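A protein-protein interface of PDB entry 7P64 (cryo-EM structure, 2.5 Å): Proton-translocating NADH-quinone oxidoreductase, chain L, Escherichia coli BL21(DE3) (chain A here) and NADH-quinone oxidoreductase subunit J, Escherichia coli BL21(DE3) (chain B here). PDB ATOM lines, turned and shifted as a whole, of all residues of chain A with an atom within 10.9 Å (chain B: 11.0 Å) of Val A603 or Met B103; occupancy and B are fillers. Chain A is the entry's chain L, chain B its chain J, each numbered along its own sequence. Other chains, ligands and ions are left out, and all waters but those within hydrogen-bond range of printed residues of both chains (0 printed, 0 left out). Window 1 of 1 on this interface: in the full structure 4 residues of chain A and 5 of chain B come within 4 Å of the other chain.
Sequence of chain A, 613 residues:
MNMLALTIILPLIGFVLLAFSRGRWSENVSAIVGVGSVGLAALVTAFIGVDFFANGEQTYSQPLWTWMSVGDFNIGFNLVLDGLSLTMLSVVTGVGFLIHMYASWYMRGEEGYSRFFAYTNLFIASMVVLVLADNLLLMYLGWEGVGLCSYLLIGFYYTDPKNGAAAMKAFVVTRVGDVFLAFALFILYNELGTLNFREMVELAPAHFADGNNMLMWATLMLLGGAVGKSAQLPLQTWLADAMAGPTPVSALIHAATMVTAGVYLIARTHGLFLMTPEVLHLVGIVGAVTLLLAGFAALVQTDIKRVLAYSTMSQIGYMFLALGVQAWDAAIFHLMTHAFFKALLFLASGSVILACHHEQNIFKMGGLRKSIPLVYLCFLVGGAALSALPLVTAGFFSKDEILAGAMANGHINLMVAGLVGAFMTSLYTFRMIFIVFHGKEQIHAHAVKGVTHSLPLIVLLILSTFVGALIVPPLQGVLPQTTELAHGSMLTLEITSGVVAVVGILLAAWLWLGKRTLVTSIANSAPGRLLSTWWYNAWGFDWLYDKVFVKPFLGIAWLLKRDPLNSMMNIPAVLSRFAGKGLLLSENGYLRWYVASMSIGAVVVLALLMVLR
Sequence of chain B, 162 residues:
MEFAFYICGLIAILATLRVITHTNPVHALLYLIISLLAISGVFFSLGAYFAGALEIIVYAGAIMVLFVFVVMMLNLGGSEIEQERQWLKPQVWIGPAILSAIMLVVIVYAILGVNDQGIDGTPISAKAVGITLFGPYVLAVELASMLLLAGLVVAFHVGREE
O of Val A595 lies within hydrogen-bond range of OG of Ser A599, at 3.1 Å. The side-chain hydroxyl (OG) of Ser A599 is in hydrogen-bond range of the backbone carbonyl oxygen (O) of Ala A596, 2.7 Å away.
Met B103 touches just one residue of chain A: Val A603 (3.7 Å). Of chain B, only Leu B99 comes within 4 Å of Ser A599. No residue of chain B comes within 4 Å of Gly A601. No residue of chain B comes within 4 Å of Ala A602. Val A604 touches none of the printed residues of chain B. No residue of chain B comes within 4 Å of Val A605. No residue of chain B comes within 4 Å of Ala A607. No residue of chain A comes within 4 Å of Ser B100. Leu B104 touches none of the printed residues of chain A. No residue of chain A comes within 4 Å of Val B105. Of chain A, only Leu A606 (3.7 Å) comes within 4 Å of Val B106. Of chain A, only Leu A606 (3.7 Å) comes within 4 Å of Ile B107. Printed residues of chain A within 4 Å of Leu B99: Ser A599 (3.3 Å), Ile A600 (3.7 Å) and Val A603 (3.8 Å). Printed residues of chain B within 4 Å of Ile A600: Leu B99. Met A598 touches none of the printed residues of chain B. The nearest residue of chain A that does not touch Met B103 is Ser A599 (4.1 Å).
Among the printed residues, pairs that only touch across the chains: Ser A599 with Leu B99, Val A603 with Met B103, Leu A606 with Ile B107, Ile A600 with Leu B99, Leu A606 with Val B106, Val A603 with Ile B102 and Val A603 with Leu B99.
Of the 18 printed residues of chain B, 5 touch a printed residue of chain A. Printed residues of chain B that touch a printed residue of chain A: Leu B99, Ile B102, Met B103, Val B106 and Ile B107. Hydrophobic or aromatic side chains of chain B that line the printed part of chain A: Leu B99, Ile B102, Met B103, Val B106 and Ile B107.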
ATOM      1  N   VAL A 595       1.440 -12.668 -18.270  1.00  0.00           N
ATOM      2  CA  VAL A 595       0.761 -13.190 -17.085  1.00  0.00           C
ATOM      3  C   VAL A 595       0.346 -14.643 -17.296  1.00  0.00           C
ATOM      4  O   VAL A 595       0.474 -15.483 -16.392  1.00  0.00           O
ATOM      5  CB  VAL A 595      -0.447 -12.302 -16.732  1.00  0.00           C
ATOM      6  CG1 VAL A 595      -1.149 -12.835 -15.505  1.00  0.00           C
ATOM      7  CG2 VAL A 595      -0.010 -10.870 -16.508  1.00  0.00           C
ATOM      8  N   ALA A 596      -0.162 -14.959 -18.493  1.00  0.00           N
ATOM      9  CA  ALA A 596      -0.569 -16.326 -18.802  1.00  0.00           C
ATOM     10  C   ALA A 596       0.614 -17.282 -18.772  1.00  0.00           C
ATOM     11  O   ALA A 596       0.488 -18.418 -18.309  1.00  0.00           O
ATOM     12  CB  ALA A 596      -1.255 -16.370 -20.166  1.00  0.00           C
ATOM     13  N   SER A 597       1.773 -16.838 -19.253  1.00  0.00           N
ATOM     14  CA  SER A 597       2.975 -17.659 -19.197  1.00  0.00           C
ATOM     15  C   SER A 597       3.471 -17.829 -17.769  1.00  0.00           C
ATOM     16  O   SER A 597       4.009 -18.886 -17.429  1.00  0.00           O
ATOM     17  CB  SER A 597       4.069 -17.051 -20.069  1.00  0.00           C
ATOM     18  OG  SER A 597       4.685 -15.961 -19.415  1.00  0.00           O
ATOM     19  N   MET A 598       3.293 -16.808 -16.923  1.00  0.00           N
ATOM     20  CA  MET A 598       3.604 -16.965 -15.504  1.00  0.00           C
ATOM     21  C   MET A 598       2.725 -18.032 -14.857  1.00  0.00           C
ATOM     22  O   MET A 598       3.215 -18.876 -14.098  1.00  0.00           O
ATOM     23  CB  MET A 598       3.435 -15.635 -14.776  1.00  0.00           C
ATOM     24  CG  MET A 598       3.955 -15.643 -13.352  1.00  0.00           C
ATOM     25  SD  MET A 598       3.758 -14.054 -12.525  1.00  0.00           S
ATOM     26  CE  MET A 598       5.015 -13.096 -13.356  1.00  0.00           C
ATOM     27  N   SER A 599       1.425 -18.017 -15.158  1.00  0.00           N
ATOM     28  CA  SER A 599       0.533 -19.028 -14.593  1.00  0.00           C
ATOM     29  C   SER A 599       0.799 -20.414 -15.175  1.00  0.00           C
ATOM     30  O   SER A 599       0.681 -21.418 -14.459  1.00  0.00           O
ATOM     31  CB  SER A 599      -0.924 -18.626 -14.805  1.00  0.00           C
ATOM     32  OG  SER A 599      -1.138 -18.157 -16.119  1.00  0.00           O
ATOM     33  N   ILE A 600       1.169 -20.486 -16.456  1.00  0.00           N
ATOM     34  CA  ILE A 600       1.556 -21.754 -17.072  1.00  0.00           C
ATOM     35  C   ILE A 600       2.795 -22.318 -16.389  1.00  0.00           C
ATOM     36  O   ILE A 600       2.858 -23.513 -16.071  1.00  0.00           O
ATOM     37  CB  ILE A 600       1.780 -21.561 -18.585  1.00  0.00           C
ATOM     38  CG1 ILE A 600       0.449 -21.520 -19.332  1.00  0.00           C
ATOM     39  CG2 ILE A 600       2.653 -22.662 -19.166  1.00  0.00           C
ATOM     40  CD1 ILE A 600       0.550 -20.907 -20.706  1.00  0.00           C
ATOM     41  N   GLY A 601       3.790 -21.464 -16.142  1.00  0.00           N
ATOM     42  CA  GLY A 601       4.987 -21.909 -15.450  1.00  0.00           C
ATOM     43  C   GLY A 601       4.719 -22.324 -14.019  1.00  0.00           C
ATOM     44  O   GLY A 601       5.349 -23.250 -13.507  1.00  0.00           O
ATOM     45  N   ALA A 602       3.781 -21.644 -13.353  1.00  0.00           N
ATOM     46  CA  ALA A 602       3.380 -22.055 -12.011  1.00  0.00           C
ATOM     47  C   ALA A 602       2.744 -23.439 -12.022  1.00  0.00           C
ATOM     48  O   ALA A 602       3.054 -24.280 -11.167  1.00  0.00           O
ATOM     49  CB  ALA A 602       2.419 -21.029 -11.415  1.00  0.00           C
ATOM     50  N   VAL A 603       1.870 -23.694 -12.998  1.00  0.00           N
ATOM     51  CA  VAL A 603       1.242 -25.005 -13.135  1.00  0.00           C
ATOM     52  C   VAL A 603       2.292 -26.074 -13.410  1.00  0.00           C
ATOM     53  O   VAL A 603       2.269 -27.155 -12.808  1.00  0.00           O
ATOM     54  CB  VAL A 603       0.170 -24.960 -14.240  1.00  0.00           C
ATOM     55  CG1 VAL A 603      -0.244 -26.359 -14.662  1.00  0.00           C
ATOM     56  CG2 VAL A 603      -1.029 -24.167 -13.773  1.00  0.00           C
ATOM     57  N   VAL A 604       3.241 -25.776 -14.299  1.00  0.00           N
ATOM     58  CA  VAL A 604       4.278 -26.739 -14.665  1.00  0.00           C
ATOM     59  C   VAL A 604       5.176 -27.052 -13.473  1.00  0.00           C
ATOM     60  O   VAL A 604       5.465 -28.223 -13.193  1.00  0.00           O
ATOM     61  CB  VAL A 604       5.081 -26.208 -15.869  1.00  0.00           C
ATOM     62  CG1 VAL A 604       6.407 -26.937 -16.013  1.00  0.00           C
ATOM     63  CG2 VAL A 604       4.267 -26.342 -17.140  1.00  0.00           C
ATOM     64  N   VAL A 605       5.601 -26.022 -12.734  1.00  0.00           N
ATOM     65  CA  VAL A 605       6.474 -26.216 -11.579  1.00  0.00           C
ATOM     66  C   VAL A 605       5.762 -27.008 -10.487  1.00  0.00           C
ATOM     67  O   VAL A 605       6.332 -27.946  -9.914  1.00  0.00           O
ATOM     68  CB  VAL A 605       6.977 -24.852 -11.066  1.00  0.00           C
ATOM     69  CG1 VAL A 605       7.485 -24.951  -9.637  1.00  0.00           C
ATOM     70  CG2 VAL A 605       8.065 -24.310 -11.977  1.00  0.00           C
ATOM     71  N   LEU A 606       4.501 -26.671 -10.201  1.00  0.00           N
ATOM     72  CA  LEU A 606       3.778 -27.381  -9.151  1.00  0.00           C
ATOM     73  C   LEU A 606       3.481 -28.823  -9.547  1.00  0.00           C
ATOM     74  O   LEU A 606       3.589 -29.730  -8.713  1.00  0.00           O
ATOM     75  CB  LEU A 606       2.492 -26.636  -8.807  1.00  0.00           C
ATOM     76  CG  LEU A 606       2.535 -25.908  -7.464  1.00  0.00           C
ATOM     77  CD1 LEU A 606       3.443 -24.700  -7.541  1.00  0.00           C
ATOM     78  CD2 LEU A 606       1.144 -25.504  -7.046  1.00  0.00           C
ATOM     79  N   ALA A 607       3.121 -29.060 -10.812  1.00  0.00           N
ATOM     80  CA  ALA A 607       2.871 -30.420 -11.274  1.00  0.00           C
ATOM     81  C   ALA A 607       4.141 -31.258 -11.240  1.00  0.00           C
ATOM     82  O   ALA A 607       4.101 -32.436 -10.869  1.00  0.00           O
ATOM     83  CB  ALA A 607       2.280 -30.395 -12.683  1.00  0.00           C
ATOM     84  N   LEU A 608       5.278 -30.662 -11.613  1.00  0.00           N
ATOM     85  CA  LEU A 608       6.550 -31.366 -11.517  1.00  0.00           C
ATOM     86  C   LEU A 608       6.898 -31.684 -10.071  1.00  0.00           C
ATOM     87  O   LEU A 608       7.413 -32.766  -9.776  1.00  0.00           O
ATOM     88  CB  LEU A 608       7.657 -30.539 -12.163  1.00  0.00           C
ATOM     89  CG  LEU A 608       7.811 -30.705 -13.672  1.00  0.00           C
ATOM     90  CD1 LEU A 608       8.811 -29.705 -14.216  1.00  0.00           C
ATOM     91  CD2 LEU A 608       8.233 -32.124 -14.002  1.00  0.00           C
ATOM     92  N   LEU A 609       6.620 -30.756  -9.153  1.00  0.00           N
ATOM     93  CA  LEU A 609       6.942 -30.995  -7.749  1.00  0.00           C
ATOM     94  C   LEU A 609       6.074 -32.097  -7.151  1.00  0.00           C
ATOM     95  O   LEU A 609       6.558 -32.900  -6.347  1.00  0.00           O
ATOM     96  CB  LEU A 609       6.804 -29.702  -6.953  1.00  0.00           C
ATOM     97  CG  LEU A 609       8.050 -28.825  -7.037  1.00  0.00           C
ATOM     98  CD1 LEU A 609       7.791 -27.474  -6.426  1.00  0.00           C
ATOM     99  CD2 LEU A 609       9.219 -29.504  -6.356  1.00  0.00           C
ATOM    100  N   MET A 610       4.791 -32.156  -7.523  1.00  0.00           N
ATOM    101  CA  MET A 610       3.955 -33.246  -7.021  1.00  0.00           C
ATOM    102  C   MET A 610       4.248 -34.568  -7.719  1.00  0.00           C
ATOM    103  O   MET A 610       3.984 -35.631  -7.147  1.00  0.00           O
ATOM    104  CB  MET A 610       2.471 -32.904  -7.140  1.00  0.00           C
ATOM    105  CG  MET A 610       2.107 -31.548  -6.593  1.00  0.00           C
ATOM    106  SD  MET A 610       2.355 -31.462  -4.812  1.00  0.00           S
ATOM    107  CE  MET A 610       3.269 -29.933  -4.686  1.00  0.00           C
ATOM    108  N   VAL A 611       4.776 -34.536  -8.943  1.00  0.00           N
ATOM    109  CA  VAL A 611       5.130 -35.782  -9.618  1.00  0.00           C
ATOM    110  C   VAL A 611       6.375 -36.398  -8.985  1.00  0.00           C
ATOM    111  O   VAL A 611       6.399 -37.592  -8.660  1.00  0.00           O
ATOM    112  CB  VAL A 611       5.307 -35.541 -11.130  1.00  0.00           C
ATOM    113  CG1 VAL A 611       6.232 -36.575 -11.750  1.00  0.00           C
ATOM    114  CG2 VAL A 611       3.961 -35.574 -11.822  1.00  0.00           C
ATOM    115  N   LEU A 612       7.413 -35.592  -8.770  1.00  0.00           N
ATOM    116  CA  LEU A 612       8.694 -36.100  -8.292  1.00  0.00           C
ATOM    117  C   LEU A 612       8.765 -36.256  -6.781  1.00  0.00           C
ATOM    118  O   LEU A 612       9.795 -36.715  -6.275  1.00  0.00           O
ATOM    119  CB  LEU A 612       9.833 -35.192  -8.761  1.00  0.00           C
ATOM    120  CG  LEU A 612       9.851 -34.832 -10.242  1.00  0.00           C
ATOM    121  CD1 LEU A 612      10.690 -33.591 -10.469  1.00  0.00           C
ATOM    122  CD2 LEU A 612      10.372 -35.993 -11.064  1.00  0.00           C
ATOM    123  N   GLY B  95      -9.464 -21.195 -22.116  1.00  0.00           N
ATOM    124  CA  GLY B  95      -8.084 -21.524 -21.848  1.00  0.00           C
ATOM    125  C   GLY B  95      -7.621 -21.161 -20.449  1.00  0.00           C
ATOM    126  O   GLY B  95      -7.169 -22.023 -19.682  1.00  0.00           O
ATOM    127  N   PRO B  96      -7.683 -19.867 -20.102  1.00  0.00           N
ATOM    128  CA  PRO B  96      -7.299 -19.455 -18.741  1.00  0.00           C
ATOM    129  C   PRO B  96      -8.126 -20.082 -17.634  1.00  0.00           C
ATOM    130  O   PRO B  96      -7.584 -20.320 -16.549  1.00  0.00           O
ATOM    131  CB  PRO B  96      -7.480 -17.935 -18.780  1.00  0.00           C
ATOM    132  CG  PRO B  96      -7.283 -17.579 -20.186  1.00  0.00           C
ATOM    133  CD  PRO B  96      -7.831 -18.701 -20.992  1.00  0.00           C
ATOM    134  N   ALA B  97      -9.413 -20.358 -17.859  1.00  0.00           N
ATOM    135  CA  ALA B  97     -10.202 -21.018 -16.821  1.00  0.00           C
ATOM    136  C   ALA B  97      -9.748 -22.454 -16.610  1.00  0.00           C
ATOM    137  O   ALA B  97      -9.704 -22.931 -15.474  1.00  0.00           O
ATOM    138  CB  ALA B  97     -11.689 -20.976 -17.160  1.00  0.00           C
ATOM    139  N   ILE B  98      -9.401 -23.159 -17.691  1.00  0.00           N
ATOM    140  CA  ILE B  98      -8.868 -24.512 -17.557  1.00  0.00           C
ATOM    141  C   ILE B  98      -7.517 -24.485 -16.851  1.00  0.00           C
ATOM    142  O   ILE B  98      -7.234 -25.331 -15.994  1.00  0.00           O
ATOM    143  CB  ILE B  98      -8.803 -25.198 -18.938  1.00  0.00           C
ATOM    144  CG1 ILE B  98     -10.126 -25.903 -19.239  1.00  0.00           C
ATOM    145  CG2 ILE B  98      -7.653 -26.192 -19.036  1.00  0.00           C
ATOM    146  CD1 ILE B  98     -10.416 -26.071 -20.710  1.00  0.00           C
ATOM    147  N   LEU B  99      -6.680 -23.496 -17.173  1.00  0.00           N
ATOM    148  CA  LEU B  99      -5.386 -23.356 -16.505  1.00  0.00           C
ATOM    149  C   LEU B  99      -5.548 -23.082 -15.013  1.00  0.00           C
ATOM    150  O   LEU B  99      -4.864 -23.693 -14.179  1.00  0.00           O
ATOM    151  CB  LEU B  99      -4.592 -22.239 -17.176  1.00  0.00           C
ATOM    152  CG  LEU B  99      -3.138 -22.024 -16.783  1.00  0.00           C
ATOM    153  CD1 LEU B  99      -2.300 -23.217 -17.182  1.00  0.00           C
ATOM    154  CD2 LEU B  99      -2.639 -20.767 -17.458  1.00  0.00           C
ATOM    155  N   SER B 100      -6.469 -22.180 -14.658  1.00  0.00           N
ATOM    156  CA  SER B 100      -6.728 -21.874 -13.256  1.00  0.00           C
ATOM    157  C   SER B 100      -7.332 -23.066 -12.527  1.00  0.00           C
ATOM    158  O   SER B 100      -7.016 -23.305 -11.361  1.00  0.00           O
ATOM    159  CB  SER B 100      -7.648 -20.661 -13.148  1.00  0.00           C
ATOM    160  OG  SER B 100      -6.903 -19.458 -13.160  1.00  0.00           O
ATOM    161  N   ALA B 101      -8.200 -23.826 -13.200  1.00  0.00           N
ATOM    162  CA  ALA B 101      -8.769 -25.023 -12.594  1.00  0.00           C
ATOM    163  C   ALA B 101      -7.702 -26.080 -12.344  1.00  0.00           C
ATOM    164  O   ALA B 101      -7.718 -26.741 -11.302  1.00  0.00           O
ATOM    165  CB  ALA B 101      -9.881 -25.581 -13.479  1.00  0.00           C
ATOM    166  N   ILE B 102      -6.769 -26.252 -13.285  1.00  0.00           N
ATOM    167  CA  ILE B 102      -5.681 -27.213 -13.102  1.00  0.00           C
ATOM    168  C   ILE B 102      -4.800 -26.804 -11.929  1.00  0.00           C
ATOM    169  O   ILE B 102      -4.440 -27.634 -11.080  1.00  0.00           O
ATOM    170  CB  ILE B 102      -4.870 -27.352 -14.406  1.00  0.00           C
ATOM    171  CG1 ILE B 102      -5.665 -28.137 -15.447  1.00  0.00           C
ATOM    172  CG2 ILE B 102      -3.541 -28.040 -14.154  1.00  0.00           C
ATOM    173  CD1 ILE B 102      -5.150 -27.961 -16.852  1.00  0.00           C
ATOM    174  N   MET B 103      -4.465 -25.513 -11.847  1.00  0.00           N
ATOM    175  CA  MET B 103      -3.672 -25.024 -10.721  1.00  0.00           C
ATOM    176  C   MET B 103      -4.415 -25.183  -9.401  1.00  0.00           C
ATOM    177  O   MET B 103      -3.809 -25.528  -8.381  1.00  0.00           O
ATOM    178  CB  MET B 103      -3.285 -23.569 -10.952  1.00  0.00           C
ATOM    179  CG  MET B 103      -2.335 -22.996  -9.916  1.00  0.00           C
ATOM    180  SD  MET B 103      -1.804 -21.308 -10.276  1.00  0.00           S
ATOM    181  CE  MET B 103      -2.586 -21.015 -11.863  1.00  0.00           C
ATOM    182  N   LEU B 104      -5.729 -24.951  -9.405  1.00  0.00           N
ATOM    183  CA  LEU B 104      -6.524 -25.127  -8.195  1.00  0.00           C
ATOM    184  C   LEU B 104      -6.554 -26.584  -7.755  1.00  0.00           C
ATOM    185  O   LEU B 104      -6.465 -26.873  -6.559  1.00  0.00           O
ATOM    186  CB  LEU B 104      -7.940 -24.605  -8.418  1.00  0.00           C
ATOM    187  CG  LEU B 104      -8.881 -24.723  -7.221  1.00  0.00           C
ATOM    188  CD1 LEU B 104      -8.344 -23.908  -6.062  1.00  0.00           C
ATOM    189  CD2 LEU B 104     -10.280 -24.280  -7.590  1.00  0.00           C
ATOM    190  N   VAL B 105      -6.676 -27.518  -8.704  1.00  0.00           N
ATOM    191  CA  VAL B 105      -6.669 -28.940  -8.355  1.00  0.00           C
ATOM    192  C   VAL B 105      -5.317 -29.350  -7.786  1.00  0.00           C
ATOM    193  O   VAL B 105      -5.248 -30.097  -6.802  1.00  0.00           O
ATOM    194  CB  VAL B 105      -7.073 -29.804  -9.567  1.00  0.00           C
ATOM    195  CG1 VAL B 105      -6.980 -31.281  -9.229  1.00  0.00           C
ATOM    196  CG2 VAL B 105      -8.503 -29.507  -9.960  1.00  0.00           C
ATOM    197  N   VAL B 106      -4.223 -28.849  -8.369  1.00  0.00           N
ATOM    198  CA  VAL B 106      -2.891 -29.178  -7.851  1.00  0.00           C
ATOM    199  C   VAL B 106      -2.701 -28.619  -6.441  1.00  0.00           C
ATOM    200  O   VAL B 106      -2.225 -29.323  -5.535  1.00  0.00           O
ATOM    201  CB  VAL B 106      -1.801 -28.674  -8.815  1.00  0.00           C
ATOM    202  CG1 VAL B 106      -0.429 -28.831  -8.194  1.00  0.00           C
ATOM    203  CG2 VAL B 106      -1.865 -29.428 -10.128  1.00  0.00           C
ATOM    204  N   ILE B 107      -3.102 -27.363  -6.223  1.00  0.00           N
ATOM    205  CA  ILE B 107      -2.958 -26.737  -4.910  1.00  0.00           C
ATOM    206  C   ILE B 107      -3.835 -27.437  -3.875  1.00  0.00           C
ATOM    207  O   ILE B 107      -3.405 -27.672  -2.742  1.00  0.00           O
ATOM    208  CB  ILE B 107      -3.267 -25.230  -5.004  1.00  0.00           C
ATOM    209  CG1 ILE B 107      -2.177 -24.509  -5.792  1.00  0.00           C
ATOM    210  CG2 ILE B 107      -3.346 -24.599  -3.634  1.00  0.00           C
ATOM    211  CD1 ILE B 107      -2.533 -23.087  -6.155  1.00  0.00           C
ATOM    212  N   VAL B 108      -5.062 -27.809  -4.252  1.00  0.00           N
ATOM    213  CA  VAL B 108      -5.969 -28.486  -3.330  1.00  0.00           C
ATOM    214  C   VAL B 108      -5.454 -29.882  -2.992  1.00  0.00           C
ATOM    215  O   VAL B 108      -5.546 -30.327  -1.841  1.00  0.00           O
ATOM    216  CB  VAL B 108      -7.392 -28.510  -3.928  1.00  0.00           C
ATOM    217  CG1 VAL B 108      -8.238 -29.636  -3.348  1.00  0.00           C
ATOM    218  CG2 VAL B 108      -8.075 -27.175  -3.702  1.00  0.00           C
ATOM    219  N   TYR B 109      -4.884 -30.583  -3.977  1.00  0.00           N
ATOM    220  CA  TYR B 109      -4.286 -31.887  -3.712  1.00  0.00           C
ATOM    221  C   TYR B 109      -3.110 -31.769  -2.753  1.00  0.00           C
ATOM    222  O   TYR B 109      -2.917 -32.629  -1.885  1.00  0.00           O
ATOM    223  CB  TYR B 109      -3.844 -32.541  -5.021  1.00  0.00           C
ATOM    224  CG  TYR B 109      -2.969 -33.757  -4.824  1.00  0.00           C
ATOM    225  CD1 TYR B 109      -3.507 -34.957  -4.384  1.00  0.00           C
ATOM    226  CD2 TYR B 109      -1.602 -33.702  -5.071  1.00  0.00           C
ATOM    227  CE1 TYR B 109      -2.713 -36.072  -4.199  1.00  0.00           C
ATOM    228  CE2 TYR B 109      -0.800 -34.808  -4.886  1.00  0.00           C
ATOM    229  CZ  TYR B 109      -1.360 -35.990  -4.451  1.00  0.00           C
ATOM    230  OH  TYR B 109      -0.563 -37.095  -4.267  1.00  0.00           O
ATOM    231  N   ALA B 110      -2.307 -30.713  -2.898  1.00  0.00           N
ATOM    232  CA  ALA B 110      -1.230 -30.478  -1.942  1.00  0.00           C
ATOM    233  C   ALA B 110      -1.772 -30.115  -0.563  1.00  0.00           C
ATOM    234  O   ALA B 110      -1.185 -30.492   0.457  1.00  0.00           O
ATOM    235  CB  ALA B 110      -0.304 -29.383  -2.458  1.00  0.00           C
ATOM    236  N   ILE B 111      -2.883 -29.377  -0.517  1.00  0.00           N
ATOM    237  CA  ILE B 111      -3.457 -28.930   0.751  1.00  0.00           C
ATOM    238  C   ILE B 111      -4.015 -30.109   1.538  1.00  0.00           C
ATOM    239  O   ILE B 111      -3.786 -30.228   2.747  1.00  0.00           O
ATOM    240  CB  ILE B 111      -4.532 -27.855   0.492  1.00  0.00           C
ATOM    241  CG1 ILE B 111      -3.890 -26.493   0.249  1.00  0.00           C
ATOM    242  CG2 ILE B 111      -5.507 -27.747   1.651  1.00  0.00           C
ATOM    243  CD1 ILE B 111      -4.836 -25.488  -0.357  1.00  0.00           C
ATOM    244  N   LEU B 112      -4.728 -31.012   0.862  1.00  0.00           N
ATOM    245  CA  LEU B 112      -5.421 -32.111   1.528  1.00  0.00           C
ATOM    246  C   LEU B 112      -4.480 -33.132   2.155  1.00  0.00           C
ATOM    247  O   LEU B 112      -4.933 -33.944   2.967  1.00  0.00           O
ATOM    248  CB  LEU B 112      -6.352 -32.815   0.543  1.00  0.00           C
ATOM    249  CG  LEU B 112      -7.601 -32.042   0.120  1.00  0.00           C
ATOM    250  CD1 LEU B 112      -8.246 -32.697  -1.088  1.00  0.00           C
ATOM    251  CD2 LEU B 112      -8.585 -31.945   1.269  1.00  0.00           C
